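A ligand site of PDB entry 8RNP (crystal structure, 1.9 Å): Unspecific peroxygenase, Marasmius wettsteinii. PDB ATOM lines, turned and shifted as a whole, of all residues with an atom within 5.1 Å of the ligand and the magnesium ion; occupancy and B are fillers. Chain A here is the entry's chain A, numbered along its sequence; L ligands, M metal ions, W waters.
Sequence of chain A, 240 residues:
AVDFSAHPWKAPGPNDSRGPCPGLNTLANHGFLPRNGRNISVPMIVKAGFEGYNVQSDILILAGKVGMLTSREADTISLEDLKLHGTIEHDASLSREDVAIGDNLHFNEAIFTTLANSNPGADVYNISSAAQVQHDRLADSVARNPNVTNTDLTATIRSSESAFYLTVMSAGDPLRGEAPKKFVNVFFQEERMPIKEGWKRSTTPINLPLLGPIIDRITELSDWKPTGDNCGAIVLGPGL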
ATOM      1  N   PRO A  20      34.920  -2.996 -22.859  1.00  0.00           N
ATOM      2  CA  PRO A  20      34.153  -4.233 -22.677  1.00  0.00           C
ATOM      3  C   PRO A  20      32.945  -4.365 -23.611  1.00  0.00           C
ATOM      4  O   PRO A  20      32.239  -5.377 -23.536  1.00  0.00           O
ATOM      5  CB  PRO A  20      33.721  -4.083 -21.223  1.00  0.00           C
ATOM      6  CG  PRO A  20      33.421  -2.601 -21.096  1.00  0.00           C
ATOM      7  CD  PRO A  20      34.428  -1.916 -22.003  1.00  0.00           C
ATOM      8  N   CYS A  21      32.746  -3.370 -24.475  1.00  0.00           N
ATOM      9  CA  CYS A  21      31.652  -3.330 -25.444  1.00  0.00           C
ATOM     10  C   CYS A  21      32.103  -3.751 -26.852  1.00  0.00           C
ATOM     11  O   CYS A  21      32.827  -3.017 -27.524  1.00  0.00           O
ATOM     12  CB  CYS A  21      31.097  -1.924 -25.610  1.00  0.00           C
ATOM     13  SG  CYS A  21      29.728  -1.863 -26.794  1.00  0.00           S
ATOM     14  N   PRO A  22      31.695  -4.935 -27.345  1.00  0.00           N
ATOM     15  CA  PRO A  22      31.989  -5.337 -28.722  1.00  0.00           C
ATOM     16  C   PRO A  22      31.425  -4.389 -29.780  1.00  0.00           C
ATOM     17  O   PRO A  22      32.013  -4.259 -30.847  1.00  0.00           O
ATOM     18  CB  PRO A  22      31.374  -6.738 -28.839  1.00  0.00           C
ATOM     19  CG  PRO A  22      30.294  -6.772 -27.771  1.00  0.00           C
ATOM     20  CD  PRO A  22      30.864  -5.923 -26.639  1.00  0.00           C
ATOM     21  N   GLY A  23      30.277  -3.756 -29.490  1.00  0.00           N
ATOM     22  CA  GLY A  23      29.636  -2.826 -30.407  1.00  0.00           C
ATOM     23  C   GLY A  23      30.530  -1.637 -30.751  1.00  0.00           C
ATOM     24  O   GLY A  23      30.728  -1.305 -31.929  1.00  0.00           O
ATOM     25  N   LEU A  24      31.088  -1.005 -29.713  1.00  0.00           N
ATOM     26  CA  LEU A  24      31.947   0.157 -29.865  1.00  0.00           C
ATOM     27  C   LEU A  24      33.339  -0.271 -30.348  1.00  0.00           C
ATOM     28  O   LEU A  24      33.912   0.416 -31.178  1.00  0.00           O
ATOM     29  CB  LEU A  24      32.036   0.939 -28.558  1.00  0.00           C
ATOM     30  CG  LEU A  24      30.726   1.585 -28.083  1.00  0.00           C
ATOM     31  CD1 LEU A  24      30.995   2.423 -26.826  1.00  0.00           C
ATOM     32  CD2 LEU A  24      30.058   2.438 -29.141  1.00  0.00           C
ATOM     33  N   ILE A  45      29.834   8.836 -31.147  1.00  0.00           N
ATOM     34  CA  ILE A  45      29.199   7.543 -30.970  1.00  0.00           C
ATOM     35  C   ILE A  45      27.892   7.487 -31.778  1.00  0.00           C
ATOM     36  O   ILE A  45      27.595   6.486 -32.418  1.00  0.00           O
ATOM     37  CB  ILE A  45      28.954   7.233 -29.473  1.00  0.00           C
ATOM     38  CG1 ILE A  45      30.274   7.006 -28.726  1.00  0.00           C
ATOM     39  CG2 ILE A  45      28.020   6.029 -29.331  1.00  0.00           C
ATOM     40  CD1 ILE A  45      30.145   6.841 -27.225  1.00  0.00           C
ATOM     41  N   TYR A  53      25.754   0.675 -38.078  1.00  0.00           N
ATOM     42  CA  TYR A  53      24.778  -0.317 -37.655  1.00  0.00           C
ATOM     43  C   TYR A  53      23.317   0.090 -37.905  1.00  0.00           C
ATOM     44  O   TYR A  53      22.440  -0.760 -37.801  1.00  0.00           O
ATOM     45  CB  TYR A  53      24.872  -0.568 -36.144  1.00  0.00           C
ATOM     46  CG  TYR A  53      26.201  -1.090 -35.619  1.00  0.00           C
ATOM     47  CD1 TYR A  53      26.921  -2.051 -36.310  1.00  0.00           C
ATOM     48  CD2 TYR A  53      26.681  -0.659 -34.387  1.00  0.00           C
ATOM     49  CE1 TYR A  53      28.128  -2.533 -35.801  1.00  0.00           C
ATOM     50  CE2 TYR A  53      27.891  -1.119 -33.883  1.00  0.00           C
ATOM     51  CZ  TYR A  53      28.610  -2.066 -34.595  1.00  0.00           C
ATOM     52  OH  TYR A  53      29.767  -2.532 -34.073  1.00  0.00           O
ATOM     53  N   VAL A  55      21.839   2.107 -35.882  1.00  0.00           N
ATOM     54  CA  VAL A  55      21.311   2.346 -34.545  1.00  0.00           C
ATOM     55  C   VAL A  55      21.122   3.862 -34.416  1.00  0.00           C
ATOM     56  O   VAL A  55      22.051   4.632 -34.691  1.00  0.00           O
ATOM     57  CB  VAL A  55      22.248   1.791 -33.460  1.00  0.00           C
ATOM     58  CG1 VAL A  55      21.762   2.152 -32.057  1.00  0.00           C
ATOM     59  CG2 VAL A  55      22.410   0.282 -33.579  1.00  0.00           C
ATOM     60  N   ILE A  59      18.840   5.758 -28.394  1.00  0.00           N
ATOM     61  CA  ILE A  59      19.471   4.864 -27.451  1.00  0.00           C
ATOM     62  C   ILE A  59      20.948   5.232 -27.266  1.00  0.00           C
ATOM     63  O   ILE A  59      21.483   5.020 -26.179  1.00  0.00           O
ATOM     64  CB  ILE A  59      19.271   3.400 -27.878  1.00  0.00           C
ATOM     65  CG1 ILE A  59      19.839   2.480 -26.802  1.00  0.00           C
ATOM     66  CG2 ILE A  59      19.861   3.130 -29.259  1.00  0.00           C
ATOM     67  CD1 ILE A  59      19.315   1.054 -26.880  1.00  0.00           C
ATOM     68  N   LEU A  60      21.589   5.776 -28.305  1.00  0.00           N
ATOM     69  CA  LEU A  60      23.017   6.076 -28.257  1.00  0.00           C
ATOM     70  C   LEU A  60      23.275   7.313 -27.410  1.00  0.00           C
ATOM     71  O   LEU A  60      24.317   7.401 -26.766  1.00  0.00           O
ATOM     72  CB  LEU A  60      23.605   6.227 -29.657  1.00  0.00           C
ATOM     73  CG  LEU A  60      23.594   4.955 -30.496  1.00  0.00           C
ATOM     74  CD1 LEU A  60      24.198   5.164 -31.877  1.00  0.00           C
ATOM     75  CD2 LEU A  60      24.305   3.819 -29.777  1.00  0.00           C
ATOM     76  N   ALA A  63      22.584   5.892 -23.567  1.00  0.00           N
ATOM     77  CA  ALA A  63      23.715   5.088 -23.147  1.00  0.00           C
ATOM     78  C   ALA A  63      25.029   5.867 -23.182  1.00  0.00           C
ATOM     79  O   ALA A  63      25.884   5.713 -22.303  1.00  0.00           O
ATOM     80  CB  ALA A  63      23.812   3.871 -24.047  1.00  0.00           C
ATOM     81  N   GLY A  64      25.199   6.676 -24.246  1.00  0.00           N
ATOM     82  CA  GLY A  64      26.435   7.428 -24.424  1.00  0.00           C
ATOM     83  C   GLY A  64      26.745   8.328 -23.225  1.00  0.00           C
ATOM     84  O   GLY A  64      27.882   8.401 -22.764  1.00  0.00           O
ATOM     85  N   GLY A  67      27.799   6.452 -20.277  1.00  0.00           N
ATOM     86  CA  GLY A  67      29.174   6.044 -20.483  1.00  0.00           C
ATOM     87  C   GLY A  67      30.197   7.148 -20.233  1.00  0.00           C
ATOM     88  O   GLY A  67      31.319   6.861 -19.805  1.00  0.00           O
ATOM     89  N   LEU A  82      35.226   2.459 -20.150  1.00  0.00           N
ATOM     90  CA  LEU A  82      33.884   1.899 -19.983  1.00  0.00           C
ATOM     91  C   LEU A  82      33.909   0.652 -19.105  1.00  0.00           C
ATOM     92  O   LEU A  82      32.852   0.130 -18.762  1.00  0.00           O
ATOM     93  CB  LEU A  82      33.263   1.589 -21.348  1.00  0.00           C
ATOM     94  CG  LEU A  82      32.882   2.800 -22.200  1.00  0.00           C
ATOM     95  CD1 LEU A  82      32.445   2.344 -23.574  1.00  0.00           C
ATOM     96  CD2 LEU A  82      31.782   3.607 -21.516  1.00  0.00           C
ATOM     97  N   ILE A  88      28.079   1.213 -16.300  1.00  0.00           N
ATOM     98  CA  ILE A  88      27.369   0.304 -17.184  1.00  0.00           C
ATOM     99  C   ILE A  88      27.893  -1.106 -17.000  1.00  0.00           C
ATOM    100  O   ILE A  88      27.092  -2.044 -16.899  1.00  0.00           O
ATOM    101  CB  ILE A  88      27.430   0.775 -18.646  1.00  0.00           C
ATOM    102  CG1 ILE A  88      26.680   2.097 -18.830  1.00  0.00           C
ATOM    103  CG2 ILE A  88      26.889  -0.288 -19.604  1.00  0.00           C
ATOM    104  CD1 ILE A  88      26.965   2.764 -20.159  1.00  0.00           C
ATOM    105  N   GLU A  89      29.217  -1.272 -16.924  1.00  0.00           N
ATOM    106  CA  GLU A  89      29.803  -2.611 -16.843  1.00  0.00           C
ATOM    107  C   GLU A  89      29.209  -3.346 -15.639  1.00  0.00           C
ATOM    108  O   GLU A  89      28.994  -2.772 -14.583  1.00  0.00           O
ATOM    109  CB  GLU A  89      31.323  -2.520 -16.804  1.00  0.00           C
ATOM    110  CG  GLU A  89      32.018  -3.861 -17.031  1.00  0.00           C
ATOM    111  CD  GLU A  89      31.995  -4.834 -15.874  1.00  0.00           C
ATOM    112  OE1 GLU A  89      32.219  -4.350 -14.752  1.00  0.00           O
ATOM    113  OE2 GLU A  89      31.836  -6.069 -16.101  1.00  0.00           O
ATOM    114  N   HIS A  90      28.972  -4.642 -15.825  1.00  0.00           N
ATOM    115  CA  HIS A  90      28.203  -5.434 -14.895  1.00  0.00           C
ATOM    116  C   HIS A  90      28.675  -6.881 -14.912  1.00  0.00           C
ATOM    117  O   HIS A  90      29.259  -7.345 -15.895  1.00  0.00           O
ATOM    118  CB  HIS A  90      26.723  -5.374 -15.312  1.00  0.00           C
ATOM    119  CG  HIS A  90      26.486  -5.828 -16.715  1.00  0.00           C
ATOM    120  ND1 HIS A  90      26.614  -7.152 -17.072  1.00  0.00           N
ATOM    121  CD2 HIS A  90      26.194  -5.154 -17.844  1.00  0.00           C
ATOM    122  CE1 HIS A  90      26.350  -7.279 -18.378  1.00  0.00           C
ATOM    123  NE2 HIS A  90      26.086  -6.081 -18.863  1.00  0.00           N
ATOM    124  N   ASP A  91      28.345  -7.597 -13.826  1.00  0.00           N
ATOM    125  CA  ASP A  91      28.564  -9.032 -13.724  1.00  0.00           C
ATOM    126  C   ASP A  91      27.685  -9.773 -14.723  1.00  0.00           C
ATOM    127  O   ASP A  91      26.700  -9.224 -15.226  1.00  0.00           O
ATOM    128  CB  ASP A  91      28.305  -9.485 -12.284  1.00  0.00           C
ATOM    129  CG  ASP A  91      29.277  -8.932 -11.245  1.00  0.00           C
ATOM    130  OD1 ASP A  91      30.420  -8.593 -11.627  1.00  0.00           O
ATOM    131  OD2 ASP A  91      28.871  -8.784 -10.060  1.00  0.00           O
ATOM    132  N   SER A  93      28.375 -10.927 -17.712  1.00  0.00           N
ATOM    133  CA  SER A  93      28.593 -10.566 -19.099  1.00  0.00           C
ATOM    134  C   SER A  93      28.581 -11.820 -19.980  1.00  0.00           C
ATOM    135  O   SER A  93      28.788 -12.927 -19.504  1.00  0.00           O
ATOM    136  CB  SER A  93      29.884  -9.821 -19.231  1.00  0.00           C
ATOM    137  OG  SER A  93      29.774  -8.504 -18.721  1.00  0.00           O
ATOM    138  N   LEU A  94      28.342 -11.622 -21.278  1.00  0.00           N
ATOM    139  CA  LEU A  94      28.276 -12.696 -22.262  1.00  0.00           C
ATOM    140  C   LEU A  94      29.658 -13.201 -22.663  1.00  0.00           C
ATOM    141  O   LEU A  94      29.760 -14.351 -23.087  1.00  0.00           O
ATOM    142  CB  LEU A  94      27.526 -12.200 -23.495  1.00  0.00           C
ATOM    143  CG  LEU A  94      26.079 -11.767 -23.273  1.00  0.00           C
ATOM    144  CD1 LEU A  94      25.584 -10.949 -24.447  1.00  0.00           C
ATOM    145  CD2 LEU A  94      25.219 -13.002 -23.057  1.00  0.00           C
ATOM    146  N   SER A  95      30.677 -12.337 -22.596  1.00  0.00           N
ATOM    147  CA  SER A  95      31.961 -12.632 -23.216  1.00  0.00           C
ATOM    148  C   SER A  95      33.125 -12.176 -22.341  1.00  0.00           C
ATOM    149  O   SER A  95      34.278 -12.364 -22.733  1.00  0.00           O
ATOM    150  CB  SER A  95      32.063 -12.010 -24.607  1.00  0.00           C
ATOM    151  OG  SER A  95      32.077 -10.593 -24.569  1.00  0.00           O
ATOM    152  N   ARG A  96      32.836 -11.560 -21.189  1.00  0.00           N
ATOM    153  CA  ARG A  96      33.864 -11.132 -20.238  1.00  0.00           C
ATOM    154  C   ARG A  96      33.602 -11.802 -18.887  1.00  0.00           C
ATOM    155  O   ARG A  96      32.505 -12.287 -18.646  1.00  0.00           O
ATOM    156  CB  ARG A  96      33.846  -9.611 -20.049  1.00  0.00           C
ATOM    157  CG  ARG A  96      34.680  -8.804 -21.046  1.00  0.00           C
ATOM    158  CD  ARG A  96      34.197  -8.901 -22.495  1.00  0.00           C
ATOM    159  NE  ARG A  96      34.858  -7.905 -23.335  1.00  0.00           N
ATOM    160  CZ  ARG A  96      34.838  -7.856 -24.672  1.00  0.00           C
ATOM    161  NH1 ARG A  96      34.103  -8.696 -25.374  1.00  0.00           N
ATOM    162  NH2 ARG A  96      35.565  -6.955 -25.308  1.00  0.00           N
ATOM    163  N   GLU A  97      34.615 -11.776 -18.022  1.00  0.00           N
ATOM    164  CA  GLU A  97      34.509 -12.301 -16.658  1.00  0.00           C
ATOM    165  C   GLU A  97      34.090 -11.198 -15.696  1.00  0.00           C
ATOM    166  O   GLU A  97      34.325 -10.016 -15.949  1.00  0.00           O
ATOM    167  CB  GLU A  97      35.852 -12.841 -16.142  1.00  0.00           C
ATOM    168  CG  GLU A  97      36.510 -13.850 -17.085  1.00  0.00           C
ATOM    169  CD  GLU A  97      37.893 -14.319 -16.671  1.00  0.00           C
ATOM    170  OE1 GLU A  97      38.739 -13.480 -16.331  1.00  0.00           O
ATOM    171  OE2 GLU A  97      38.126 -15.545 -16.767  1.00  0.00           O
ATOM    172  N   ASN A 104      37.370  -8.102 -16.618  1.00  0.00           N
ATOM    173  CA  ASN A 104      36.046  -7.643 -17.018  1.00  0.00           C
ATOM    174  C   ASN A 104      36.112  -6.827 -18.309  1.00  0.00           C
ATOM    175  O   ASN A 104      35.110  -6.228 -18.698  1.00  0.00           O
ATOM    176  CB  ASN A 104      35.345  -6.825 -15.930  1.00  0.00           C
ATOM    177  CG  ASN A 104      35.932  -5.450 -15.731  1.00  0.00           C
ATOM    178  OD1 ASN A 104      37.093  -5.201 -16.067  1.00  0.00           O
ATOM    179  ND2 ASN A 104      35.144  -4.547 -15.185  1.00  0.00           N
ATOM    180  N   GLU A 161      21.764  -5.540 -24.200  1.00  0.00           N
ATOM    181  CA  GLU A 161      22.948  -5.955 -24.902  1.00  0.00           C
ATOM    182  C   GLU A 161      22.621  -7.171 -25.766  1.00  0.00           C
ATOM    183  O   GLU A 161      23.080  -7.224 -26.908  1.00  0.00           O
ATOM    184  CB  GLU A 161      24.093  -6.134 -23.891  1.00  0.00           C
ATOM    185  CG  GLU A 161      24.468  -4.793 -23.260  1.00  0.00           C
ATOM    186  CD  GLU A 161      25.252  -4.813 -21.950  1.00  0.00           C
ATOM    187  OE1 GLU A 161      25.381  -5.889 -21.326  1.00  0.00           O
ATOM    188  OE2 GLU A 161      25.777  -3.732 -21.602  1.00  0.00           O
ATOM    189  N   PHE A 164      20.860  -6.041 -28.701  1.00  0.00           N
ATOM    190  CA  PHE A 164      21.793  -5.453 -29.650  1.00  0.00           C
ATOM    191  C   PHE A 164      22.390  -6.519 -30.565  1.00  0.00           C
ATOM    192  O   PHE A 164      22.383  -6.371 -31.775  1.00  0.00           O
ATOM    193  CB  PHE A 164      22.897  -4.683 -28.944  1.00  0.00           C
ATOM    194  CG  PHE A 164      22.669  -3.204 -28.783  1.00  0.00           C
ATOM    195  CD1 PHE A 164      22.117  -2.454 -29.818  1.00  0.00           C
ATOM    196  CD2 PHE A 164      23.077  -2.557 -27.633  1.00  0.00           C
ATOM    197  CE1 PHE A 164      21.951  -1.080 -29.683  1.00  0.00           C
ATOM    198  CE2 PHE A 164      22.888  -1.184 -27.497  1.00  0.00           C
ATOM    199  CZ  PHE A 164      22.345  -0.454 -28.531  1.00  0.00           C
ATOM    200  N   TYR A 165      22.956  -7.596 -30.027  1.00  0.00           N
ATOM    201  CA  TYR A 165      23.596  -8.556 -30.902  1.00  0.00           C
ATOM    202  C   TYR A 165      22.571  -9.191 -31.836  1.00  0.00           C
ATOM    203  O   TYR A 165      22.897  -9.447 -33.001  1.00  0.00           O
ATOM    204  CB  TYR A 165      24.499  -9.523 -30.126  1.00  0.00           C
ATOM    205  CG  TYR A 165      23.868 -10.718 -29.423  1.00  0.00           C
ATOM    206  CD1 TYR A 165      23.366 -11.805 -30.132  1.00  0.00           C
ATOM    207  CD2 TYR A 165      23.896 -10.817 -28.037  1.00  0.00           C
ATOM    208  CE1 TYR A 165      22.811 -12.895 -29.485  1.00  0.00           C
ATOM    209  CE2 TYR A 165      23.359 -11.908 -27.381  1.00  0.00           C
ATOM    210  CZ  TYR A 165      22.819 -12.953 -28.100  1.00  0.00           C
ATOM    211  OH  TYR A 165      22.324 -14.049 -27.414  1.00  0.00           O
ATOM    212  N   VAL A 168      21.566  -5.957 -34.472  1.00  0.00           N
ATOM    213  CA  VAL A 168      22.566  -5.292 -35.273  1.00  0.00           C
ATOM    214  C   VAL A 168      23.228  -6.289 -36.223  1.00  0.00           C
ATOM    215  O   VAL A 168      23.574  -5.933 -37.338  1.00  0.00           O
ATOM    216  CB  VAL A 168      23.579  -4.575 -34.351  1.00  0.00           C
ATOM    217  CG1 VAL A 168      24.865  -4.212 -35.065  1.00  0.00           C
ATOM    218  CG2 VAL A 168      22.964  -3.327 -33.711  1.00  0.00           C
ATOM    219  N   PHE A 187      31.414 -11.128 -34.612  1.00  0.00           N
ATOM    220  CA  PHE A 187      31.230  -9.879 -33.904  1.00  0.00           C
ATOM    221  C   PHE A 187      31.931  -9.943 -32.540  1.00  0.00           C
ATOM    222  O   PHE A 187      32.628  -9.005 -32.151  1.00  0.00           O
ATOM    223  CB  PHE A 187      29.732  -9.618 -33.807  1.00  0.00           C
ATOM    224  CG  PHE A 187      29.326  -8.366 -33.045  1.00  0.00           C
ATOM    225  CD1 PHE A 187      29.542  -7.112 -33.584  1.00  0.00           C
ATOM    226  CD2 PHE A 187      28.663  -8.443 -31.834  1.00  0.00           C
ATOM    227  CE1 PHE A 187      29.168  -5.956 -32.905  1.00  0.00           C
ATOM    228  CE2 PHE A 187      28.299  -7.297 -31.153  1.00  0.00           C
ATOM    229  CZ  PHE A 187      28.538  -6.053 -31.694  1.00  0.00           C
ATOM    230  N   PHE A 188      31.773 -11.064 -31.824  1.00  0.00           N
ATOM    231  CA  PHE A 188      32.292 -11.151 -30.474  1.00  0.00           C
ATOM    232  C   PHE A 188      33.768 -11.529 -30.491  1.00  0.00           C
ATOM    233  O   PHE A 188      34.567 -10.969 -29.745  1.00  0.00           O
ATOM    234  CB  PHE A 188      31.492 -12.176 -29.671  1.00  0.00           C
ATOM    235  CG  PHE A 188      30.253 -11.618 -28.978  1.00  0.00           C
ATOM    236  CD1 PHE A 188      30.357 -11.039 -27.726  1.00  0.00           C
ATOM    237  CD2 PHE A 188      28.998 -11.703 -29.565  1.00  0.00           C
ATOM    238  CE1 PHE A 188      29.228 -10.564 -27.065  1.00  0.00           C
ATOM    239  CE2 PHE A 188      27.877 -11.204 -28.918  1.00  0.00           C
ATOM    240  CZ  PHE A 188      27.994 -10.634 -27.673  1.00  0.00           C
HETATM  241  C1  LIG L   1      28.421  -4.321 -23.503  1.00  0.00           C
HETATM  242  C2  LIG L   1      28.787   0.428 -23.274  1.00  0.00           C
HETATM  243  C3  LIG L   1      26.652   0.768 -27.640  1.00  0.00           C
HETATM  244  C4  LIG L   1      26.559  -4.020 -27.939  1.00  0.00           C
HETATM  245  C5  LIG L   1      28.717  -3.065 -23.094  1.00  0.00           C
HETATM  246  C6  LIG L   1      29.376  -2.776 -21.884  1.00  0.00           C
HETATM  247  C7  LIG L   1      29.473  -1.432 -21.821  1.00  0.00           C
HETATM  248  C8  LIG L   1      28.877  -0.915 -22.978  1.00  0.00           C
HETATM  249  C9  LIG L   1      30.119  -0.612 -20.737  1.00  0.00           C
HETATM  250  C10 LIG L   1      29.905  -3.751 -20.848  1.00  0.00           C
HETATM  251  C11 LIG L   1      28.713  -4.386 -20.131  1.00  0.00           C
HETATM  252  C12 LIG L   1      29.145  -5.715 -19.571  1.00  0.00           C
HETATM  253  O1  LIG L   1      29.580  -5.827 -18.377  1.00  0.00           O
HETATM  254  O2  LIG L   1      29.092  -6.731 -20.312  1.00  0.00           O
HETATM  255  C13 LIG L   1      28.182   0.906 -24.442  1.00  0.00           C
HETATM  256  C14 LIG L   1      28.021   2.285 -24.674  1.00  0.00           C
HETATM  257  C15 LIG L   1      27.437   2.415 -25.879  1.00  0.00           C
HETATM  258  C16 LIG L   1      27.218   1.038 -26.399  1.00  0.00           C
HETATM  259  C17 LIG L   1      28.383   3.487 -23.841  1.00  0.00           C
HETATM  260  C18 LIG L   1      27.038   3.726 -26.394  1.00  0.00           C
HETATM  261  C19 LIG L   1      25.934   3.840 -27.095  1.00  0.00           C
HETATM  262  C20 LIG L   1      26.505  -0.490 -28.181  1.00  0.00           C
HETATM  263  C21 LIG L   1      26.116  -0.762 -29.496  1.00  0.00           C
HETATM  264  C22 LIG L   1      26.082  -2.140 -29.581  1.00  0.00           C
HETATM  265  C23 LIG L   1      26.467  -2.696 -28.306  1.00  0.00           C
HETATM  266  C24 LIG L   1      25.826   0.226 -30.618  1.00  0.00           C
HETATM  267  C25 LIG L   1      25.757  -2.786 -30.838  1.00  0.00           C
HETATM  268  C26 LIG L   1      25.810  -4.083 -31.078  1.00  0.00           C
HETATM  269  C27 LIG L   1      27.038  -4.463 -26.710  1.00  0.00           C
HETATM  270  C28 LIG L   1      26.999  -5.904 -26.338  1.00  0.00           C
HETATM  271  C29 LIG L   1      27.546  -5.981 -25.095  1.00  0.00           C
HETATM  272  C30 LIG L   1      27.842  -4.587 -24.715  1.00  0.00           C
HETATM  273  C31 LIG L   1      26.515  -7.090 -27.169  1.00  0.00           C
HETATM  274  C32 LIG L   1      27.669  -7.272 -24.291  1.00  0.00           C
HETATM  275  C33 LIG L   1      29.068  -7.631 -23.757  1.00  0.00           C
HETATM  276  C34 LIG L   1      29.092  -8.962 -23.030  1.00  0.00           C
HETATM  277  O3  LIG L   1      28.110  -9.304 -22.325  1.00  0.00           O
HETATM  278  O4  LIG L   1      30.112  -9.699 -23.053  1.00  0.00           O
HETATM  279  N1  LIG L   1      28.436  -1.920 -23.788  1.00  0.00           N
HETATM  280  N2  LIG L   1      27.704   0.193 -25.470  1.00  0.00           N
HETATM  281  N3  LIG L   1      26.727  -1.643 -27.505  1.00  0.00           N
HETATM  282  N4  LIG L   1      27.568  -3.721 -25.719  1.00  0.00           N
HETATM  283 FE1  LIG L   1      27.736  -1.872 -25.681  1.00  0.00          FE
HETATM  284 MG    MG M   1      30.823  -7.197 -17.452  1.00  0.00          MG
HETATM  285  O   HOH W   1      31.756  -8.957 -16.617  1.00  0.00           O
HETATM  286  O   HOH W   2      32.446  -6.910 -18.809  1.00  0.00           O
HETATM  287  O   HOH W   3      31.618  -7.077 -21.501  1.00  0.00           O
HETATM  288  O   HOH W   4      25.705  -8.596 -21.311  1.00  0.00           O
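Of the 30 residues printed, 3 come within 4 Å of the magnesium ion.
Along chain A the residues within 4 Å of the magnesium ion span positions 89 to 93.
The nearest printed residue that does not touch the magnesium ion is Asp 91 (4.4 Å).
Water W4 bridges an oxygen (O3) of the ligand and the side-chain carboxylate (OE1) of Glu 161.
Water W3 bridges O of Pro 20 (2.7 Å) and O2 of the ligand (2.8 Å).
Residues that only touch the ligand: Leu 60 (3.1 Å), Glu 161 (3.3 Å), Phe 187 (3.4 Å), Ile 88 (3.4 Å), Leu 82 (3.5 Å), Phe 164 (3.5 Å), Pro 22 (3.7 Å), Leu 24 (3.7 Å), Ala 63 (3.7 Å), Pro 20 (3.7 Å), Gly 23 (3.7 Å), Ile 45 (3.8 Å), Arg 96 (3.8 Å), Phe 188 (3.9 Å), Val 168 (3.95 Å) and Tyr 53 (3.96 Å).
22 residues have an atom within 4 Å of the ligand: Pro 20, Cys 21, Pro 22, Gly 23, Leu 24, Ile 45, Tyr 53, Leu 60, Ala 63, Leu 82, Ile 88, Glu 89, His 90, Ser 93, Leu 94, Ser 95, Arg 96, Glu 161, Phe 164, Val 168, Phe 187 and Phe 188.
The backbone NH of His 90 lies close to an oxygen (O1) of the ligand.
NE2 of His 90 sits close to O2 of the ligand, 3.4 Å away.
An iron atom (FE1) of the ligand is bound by the side-chain sulfur (SG) of Cys 21 (2.3 Å).
O3 of the ligand is in hydrogen-bond range of N of Leu 94 (2.6 Å).
N of Ser 95 lies within hydrogen-bond range of O4 of the ligand (2.7 Å).
The side-chain hydroxyl (OG) of Ser 95 lies within hydrogen-bond range of an oxygen (O4) of the ligand, 2.6 Å away.
ND2 of Asn 104 is in hydrogen-bond range of OE1 of Glu 89 (3.0 Å).
NE2 of His 90 lies within hydrogen-bond range of OE1 of Glu 161 (2.6 Å).
SG of Cys 21 lies close to N of Leu 24 (3.3 Å).
The side-chain sulfur (SG) of Cys 21 lies close to the backbone NH (N) of Gly 23 (3.3 Å).
OG of Ser 95 lies within hydrogen-bond range of NH1 of Arg 96, 2.9 Å away.
The side-chain hydroxyl of Tyr 53 lies within hydrogen-bond range of the backbone carbonyl oxygen of Gly 23 (2.7 Å).
The magnesium ion is bound by the side-chain carboxylate (OE2) of Glu 89 (2.0 Å), an oxygen (O1) of the ligand (2.1 Å), the side-chain hydroxyl (OG) of Ser 93 (2.1 Å), water W2 (2.1 Å), water W1 (2.2 Å) and the backbone carbonyl oxygen (O) of His 90 (2.2 Å).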
